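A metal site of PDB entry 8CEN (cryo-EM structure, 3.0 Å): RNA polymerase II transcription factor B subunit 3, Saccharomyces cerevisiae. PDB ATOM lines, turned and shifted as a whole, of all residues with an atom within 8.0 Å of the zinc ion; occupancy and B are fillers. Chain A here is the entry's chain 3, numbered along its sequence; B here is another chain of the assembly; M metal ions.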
ATOM      1  N   MET A  12       1.323  -7.813  22.772  1.00  0.00           N
ATOM      2  CA  MET A  12       2.108  -8.962  22.349  1.00  0.00           C
ATOM      3  C   MET A  12       3.437  -8.508  21.760  1.00  0.00           C
ATOM      4  O   MET A  12       3.569  -7.377  21.278  1.00  0.00           O
ATOM      5  CB  MET A  12       1.297  -9.825  21.354  1.00  0.00           C
ATOM      6  CG  MET A  12       0.872  -9.156  20.041  1.00  0.00           C
ATOM      7  SD  MET A  12       2.106  -8.998  18.739  1.00  0.00           S
ATOM      8  CE  MET A  12       2.243 -10.712  18.248  1.00  0.00           C
ATOM      9  N   CYS A  13       4.420  -9.411  21.807  1.00  0.00           N
ATOM     10  CA  CYS A  13       5.755  -9.142  21.279  1.00  0.00           C
ATOM     11  C   CYS A  13       5.761  -9.509  19.802  1.00  0.00           C
ATOM     12  O   CYS A  13       5.624 -10.695  19.460  1.00  0.00           O
ATOM     13  CB  CYS A  13       6.799  -9.964  22.035  1.00  0.00           C
ATOM     14  SG  CYS A  13       8.525  -9.711  21.547  1.00  0.00           S
ATOM     15  N   PRO A  14       5.930  -8.546  18.882  1.00  0.00           N
ATOM     16  CA  PRO A  14       5.906  -8.883  17.453  1.00  0.00           C
ATOM     17  C   PRO A  14       7.091  -9.705  16.983  1.00  0.00           C
ATOM     18  O   PRO A  14       6.983 -10.379  15.953  1.00  0.00           O
ATOM     19  CB  PRO A  14       5.876  -7.507  16.764  1.00  0.00           C
ATOM     20  CG  PRO A  14       5.394  -6.563  17.808  1.00  0.00           C
ATOM     21  CD  PRO A  14       5.937  -7.088  19.100  1.00  0.00           C
ATOM     22  N   ILE A  15       8.221  -9.657  17.696  1.00  0.00           N
ATOM     23  CA  ILE A  15       9.407 -10.376  17.227  1.00  0.00           C
ATOM     24  C   ILE A  15       9.237 -11.874  17.429  1.00  0.00           C
ATOM     25  O   ILE A  15       9.481 -12.672  16.509  1.00  0.00           O
ATOM     26  CB  ILE A  15      10.664  -9.842  17.941  1.00  0.00           C
ATOM     27  CG1 ILE A  15      10.831  -8.340  17.662  1.00  0.00           C
ATOM     28  CG2 ILE A  15      11.899 -10.602  17.482  1.00  0.00           C
ATOM     29  CD1 ILE A  15      10.994  -8.007  16.199  1.00  0.00           C
ATOM     30  N   CYS A  16       8.813 -12.281  18.621  1.00  0.00           N
ATOM     31  CA  CYS A  16       8.609 -13.696  18.916  1.00  0.00           C
ATOM     32  C   CYS A  16       7.166 -14.146  18.716  1.00  0.00           C
ATOM     33  O   CYS A  16       6.901 -15.349  18.846  1.00  0.00           O
ATOM     34  CB  CYS A  16       9.037 -14.020  20.348  1.00  0.00           C
ATOM     35  SG  CYS A  16       7.918 -13.399  21.611  1.00  0.00           S
ATOM     36  N   LYS A  17       6.250 -13.216  18.439  1.00  0.00           N
ATOM     37  CA  LYS A  17       4.848 -13.508  18.114  1.00  0.00           C
ATOM     38  C   LYS A  17       4.161 -14.310  19.217  1.00  0.00           C
ATOM     39  O   LYS A  17       3.685 -15.429  19.009  1.00  0.00           O
ATOM     40  CB  LYS A  17       4.736 -14.211  16.759  1.00  0.00           C
ATOM     41  CG  LYS A  17       5.103 -13.318  15.572  1.00  0.00           C
ATOM     42  CD  LYS A  17       4.133 -12.145  15.447  1.00  0.00           C
ATOM     43  CE  LYS A  17       4.392 -11.318  14.204  1.00  0.00           C
ATOM     44  NZ  LYS A  17       3.538 -10.110  14.142  1.00  0.00           N
ATOM     45  N   THR A  18       4.138 -13.738  20.415  1.00  0.00           N
ATOM     46  CA  THR A  18       3.540 -14.393  21.573  1.00  0.00           C
ATOM     47  C   THR A  18       2.606 -13.442  22.290  1.00  0.00           C
ATOM     48  O   THR A  18       2.998 -12.328  22.660  1.00  0.00           O
ATOM     49  CB  THR A  18       4.611 -14.879  22.554  1.00  0.00           C
ATOM     50  OG1 THR A  18       5.600 -13.859  22.732  1.00  0.00           O
ATOM     51  CG2 THR A  18       5.283 -16.148  22.028  1.00  0.00           C
ATOM     52  N   VAL A  26       6.265 -12.769  28.896  1.00  0.00           N
ATOM     53  CA  VAL A  26       6.764 -11.644  28.129  1.00  0.00           C
ATOM     54  C   VAL A  26       6.766 -10.393  28.990  1.00  0.00           C
ATOM     55  O   VAL A  26       5.952 -10.229  29.912  1.00  0.00           O
ATOM     56  CB  VAL A  26       5.945 -11.452  26.844  1.00  0.00           C
ATOM     57  CG1 VAL A  26       6.153 -12.612  25.887  1.00  0.00           C
ATOM     58  CG2 VAL A  26       4.472 -11.291  27.169  1.00  0.00           C
ATOM     59  N   LYS A  27       7.710  -9.487  28.699  1.00  0.00           N
ATOM     60  CA  LYS A  27       7.888  -8.283  29.488  1.00  0.00           C
ATOM     61  C   LYS A  27       8.094  -7.084  28.567  1.00  0.00           C
ATOM     62  O   LYS A  27       8.357  -7.237  27.378  1.00  0.00           O
ATOM     63  CB  LYS A  27       9.060  -8.418  30.474  1.00  0.00           C
ATOM     64  CG  LYS A  27       8.779  -9.326  31.658  1.00  0.00           C
ATOM     65  CD  LYS A  27      10.035  -9.577  32.476  1.00  0.00           C
ATOM     66  CE  LYS A  27       9.755 -10.530  33.629  1.00  0.00           C
ATOM     67  NZ  LYS A  27       9.117 -11.782  33.165  1.00  0.00           N
ATOM     68  N   ARG A  37       8.745  -2.761  21.224  1.00  0.00           N
ATOM     69  CA  ARG A  37       8.043  -3.676  22.111  1.00  0.00           C
ATOM     70  C   ARG A  37       8.635  -5.070  21.899  1.00  0.00           C
ATOM     71  O   ARG A  37       8.238  -5.791  20.976  1.00  0.00           O
ATOM     72  CB  ARG A  37       6.537  -3.648  21.848  1.00  0.00           C
ATOM     73  CG  ARG A  37       5.702  -4.688  22.601  1.00  0.00           C
ATOM     74  CD  ARG A  37       5.894  -4.601  24.107  1.00  0.00           C
ATOM     75  NE  ARG A  37       5.360  -5.764  24.797  1.00  0.00           N
ATOM     76  CZ  ARG A  37       6.097  -6.785  25.226  1.00  0.00           C
ATOM     77  NH1 ARG A  37       7.413  -6.812  25.066  1.00  0.00           N
ATOM     78  NH2 ARG A  37       5.497  -7.805  25.845  1.00  0.00           N
ATOM     79  N   ILE A  38       9.626  -5.425  22.702  1.00  0.00           N
ATOM     80  CA  ILE A  38      10.320  -6.696  22.567  1.00  0.00           C
ATOM     81  C   ILE A  38      10.388  -7.346  23.943  1.00  0.00           C
ATOM     82  O   ILE A  38      10.419  -6.657  24.979  1.00  0.00           O
ATOM     83  CB  ILE A  38      11.727  -6.514  21.929  1.00  0.00           C
ATOM     84  CG1 ILE A  38      12.322  -7.854  21.489  1.00  0.00           C
ATOM     85  CG2 ILE A  38      12.674  -5.776  22.873  1.00  0.00           C
ATOM     86  CD1 ILE A  38      13.535  -7.706  20.604  1.00  0.00           C
ATOM     87  N   CYS A  39      10.352  -8.670  23.972  1.00  0.00           N
ATOM     88  CA  CYS A  39      10.249  -9.424  25.204  1.00  0.00           C
ATOM     89  C   CYS A  39      11.618  -9.890  25.691  1.00  0.00           C
ATOM     90  O   CYS A  39      12.599  -9.906  24.954  1.00  0.00           O
ATOM     91  CB  CYS A  39       9.309 -10.626  25.027  1.00  0.00           C
ATOM     92  SG  CYS A  39      10.107 -12.063  24.306  1.00  0.00           S
ATOM     93  N   GLU A  40      11.650 -10.270  26.979  1.00  0.00           N
ATOM     94  CA  GLU A  40      12.889 -10.709  27.609  1.00  0.00           C
ATOM     95  C   GLU A  40      13.413 -11.994  26.967  1.00  0.00           C
ATOM     96  O   GLU A  40      14.632 -12.179  26.855  1.00  0.00           O
ATOM     97  CB  GLU A  40      12.651 -10.910  29.104  1.00  0.00           C
ATOM     98  CG  GLU A  40      13.886 -11.323  29.912  1.00  0.00           C
ATOM     99  CD  GLU A  40      14.974 -10.270  29.950  1.00  0.00           C
ATOM    100  OE1 GLU A  40      14.657  -9.065  29.801  1.00  0.00           O
ATOM    101  OE2 GLU A  40      16.151 -10.637  30.133  1.00  0.00           O
ATOM    102  N   SER A  41      12.506 -12.883  26.553  1.00  0.00           N
ATOM    103  CA  SER A  41      12.928 -14.105  25.874  1.00  0.00           C
ATOM    104  C   SER A  41      13.586 -13.810  24.542  1.00  0.00           C
ATOM    105  O   SER A  41      14.609 -14.411  24.198  1.00  0.00           O
ATOM    106  CB  SER A  41      11.728 -15.034  25.689  1.00  0.00           C
ATOM    107  OG  SER A  41      10.896 -14.598  24.615  1.00  0.00           O
ATOM    108  N   CYS A  42      13.032 -12.867  23.774  1.00  0.00           N
ATOM    109  CA  CYS A  42      13.653 -12.456  22.517  1.00  0.00           C
ATOM    110  C   CYS A  42      15.008 -11.795  22.760  1.00  0.00           C
ATOM    111  O   CYS A  42      15.968 -12.034  22.010  1.00  0.00           O
ATOM    112  CB  CYS A  42      12.733 -11.503  21.751  1.00  0.00           C
ATOM    113  SG  CYS A  42      11.404 -12.286  20.823  1.00  0.00           S
ATOM    114  N   VAL A  43      15.101 -10.962  23.808  1.00  0.00           N
ATOM    115  CA  VAL A  43      16.360 -10.301  24.134  1.00  0.00           C
ATOM    116  C   VAL A  43      17.429 -11.338  24.481  1.00  0.00           C
ATOM    117  O   VAL A  43      18.555 -11.296  23.955  1.00  0.00           O
ATOM    118  CB  VAL A  43      16.161  -9.300  25.280  1.00  0.00           C
ATOM    119  CG1 VAL A  43      17.499  -8.832  25.836  1.00  0.00           C
ATOM    120  CG2 VAL A  43      15.349  -8.111  24.803  1.00  0.00           C
ATOM    121  N   ARG A  45      17.439 -14.459  23.583  1.00  0.00           N
ATOM    122  CA  ARG A  45      17.726 -15.313  22.438  1.00  0.00           C
ATOM    123  C   ARG A  45      18.666 -14.631  21.452  1.00  0.00           C
ATOM    124  O   ARG A  45      19.523 -15.295  20.866  1.00  0.00           O
ATOM    125  CB  ARG A  45      16.430 -15.712  21.749  1.00  0.00           C
ATOM    126  CG  ARG A  45      16.549 -16.955  20.882  1.00  0.00           C
ATOM    127  CD  ARG A  45      15.467 -17.131  19.787  1.00  0.00           C
ATOM    128  NE  ARG A  45      15.422 -16.148  18.701  1.00  0.00           N
ATOM    129  CZ  ARG A  45      14.875 -14.935  18.759  1.00  0.00           C
ATOM    130  NH1 ARG A  45      14.176 -14.525  19.812  1.00  0.00           N
ATOM    131  NH2 ARG A  45      14.967 -14.133  17.698  1.00  0.00           N
ATOM    132  N   ILE A  46      18.512 -13.325  21.246  1.00  0.00           N
ATOM    133  CA  ILE A  46      19.319 -12.636  20.242  1.00  0.00           C
ATOM    134  C   ILE A  46      20.603 -12.076  20.831  1.00  0.00           C
ATOM    135  O   ILE A  46      21.704 -12.457  20.433  1.00  0.00           O
ATOM    136  CB  ILE A  46      18.515 -11.516  19.546  1.00  0.00           C
ATOM    137  CG1 ILE A  46      17.185 -12.051  19.022  1.00  0.00           C
ATOM    138  CG2 ILE A  46      19.321 -10.923  18.401  1.00  0.00           C
ATOM    139  CD1 ILE A  46      16.206 -10.966  18.611  1.00  0.00           C
ATOM    140  N   LYS B 110       8.807 -22.834  20.495  1.00  0.00           N
ATOM    141  CA  LYS B 110       9.873 -22.010  21.077  1.00  0.00           C
ATOM    142  C   LYS B 110      11.097 -22.849  21.395  1.00  0.00           C
ATOM    143  O   LYS B 110      12.235 -22.409  21.189  1.00  0.00           O
ATOM    144  CB  LYS B 110       9.375 -21.279  22.321  1.00  0.00           C
ATOM    145  CG  LYS B 110       8.239 -20.308  22.088  1.00  0.00           C
ATOM    146  CD  LYS B 110       8.665 -19.184  21.149  1.00  0.00           C
ATOM    147  CE  LYS B 110       9.719 -18.301  21.794  1.00  0.00           C
ATOM    148  NZ  LYS B 110       9.170 -17.581  22.972  1.00  0.00           N
ATOM    149  N   GLN B 169      11.346 -18.794  12.525  1.00  0.00           N
ATOM    150  CA  GLN B 169      10.626 -17.611  13.002  1.00  0.00           C
ATOM    151  C   GLN B 169       9.458 -17.282  12.071  1.00  0.00           C
ATOM    152  O   GLN B 169       8.370 -16.915  12.547  1.00  0.00           O
ATOM    153  CB  GLN B 169      11.579 -16.426  13.115  1.00  0.00           C
ATOM    154  CG  GLN B 169      10.959 -15.161  13.671  1.00  0.00           C
ATOM    155  CD  GLN B 169      10.443 -15.341  15.084  1.00  0.00           C
ATOM    156  OE1 GLN B 169       9.238 -15.453  15.312  1.00  0.00           O
ATOM    157  NE2 GLN B 169      11.358 -15.373  16.046  1.00  0.00           N
HETATM  158 ZN    ZN M   1       9.508 -11.766  22.068  1.00  0.00          ZN
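SG of Cys 42 lies close to NH1 of Arg 45, 3.7 Å away.
The side-chain hydroxyl (OG) of Ser 41 sits close to the side-chain sulfur (SG) of Cys 39 (2.7 Å).
The side-chain hydroxyl (OG1) of Thr 18 lies close to the side-chain sulfur (SG) of Cys 16 (2.6 Å).
O of Thr 18 is in hydrogen-bond range of N of Cys 13 (3.4 Å).
Four residues have an atom within 4 Å of the zinc ion: Cys 13, Cys 16, Cys 39 and Cys 42.
The zinc ion is bound by SG of Cys 16 (2.3 Å), SG of Cys 42 (2.3 Å), SG of Cys 39 (2.3 Å) and SG of Cys 13 (2.3 Å).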
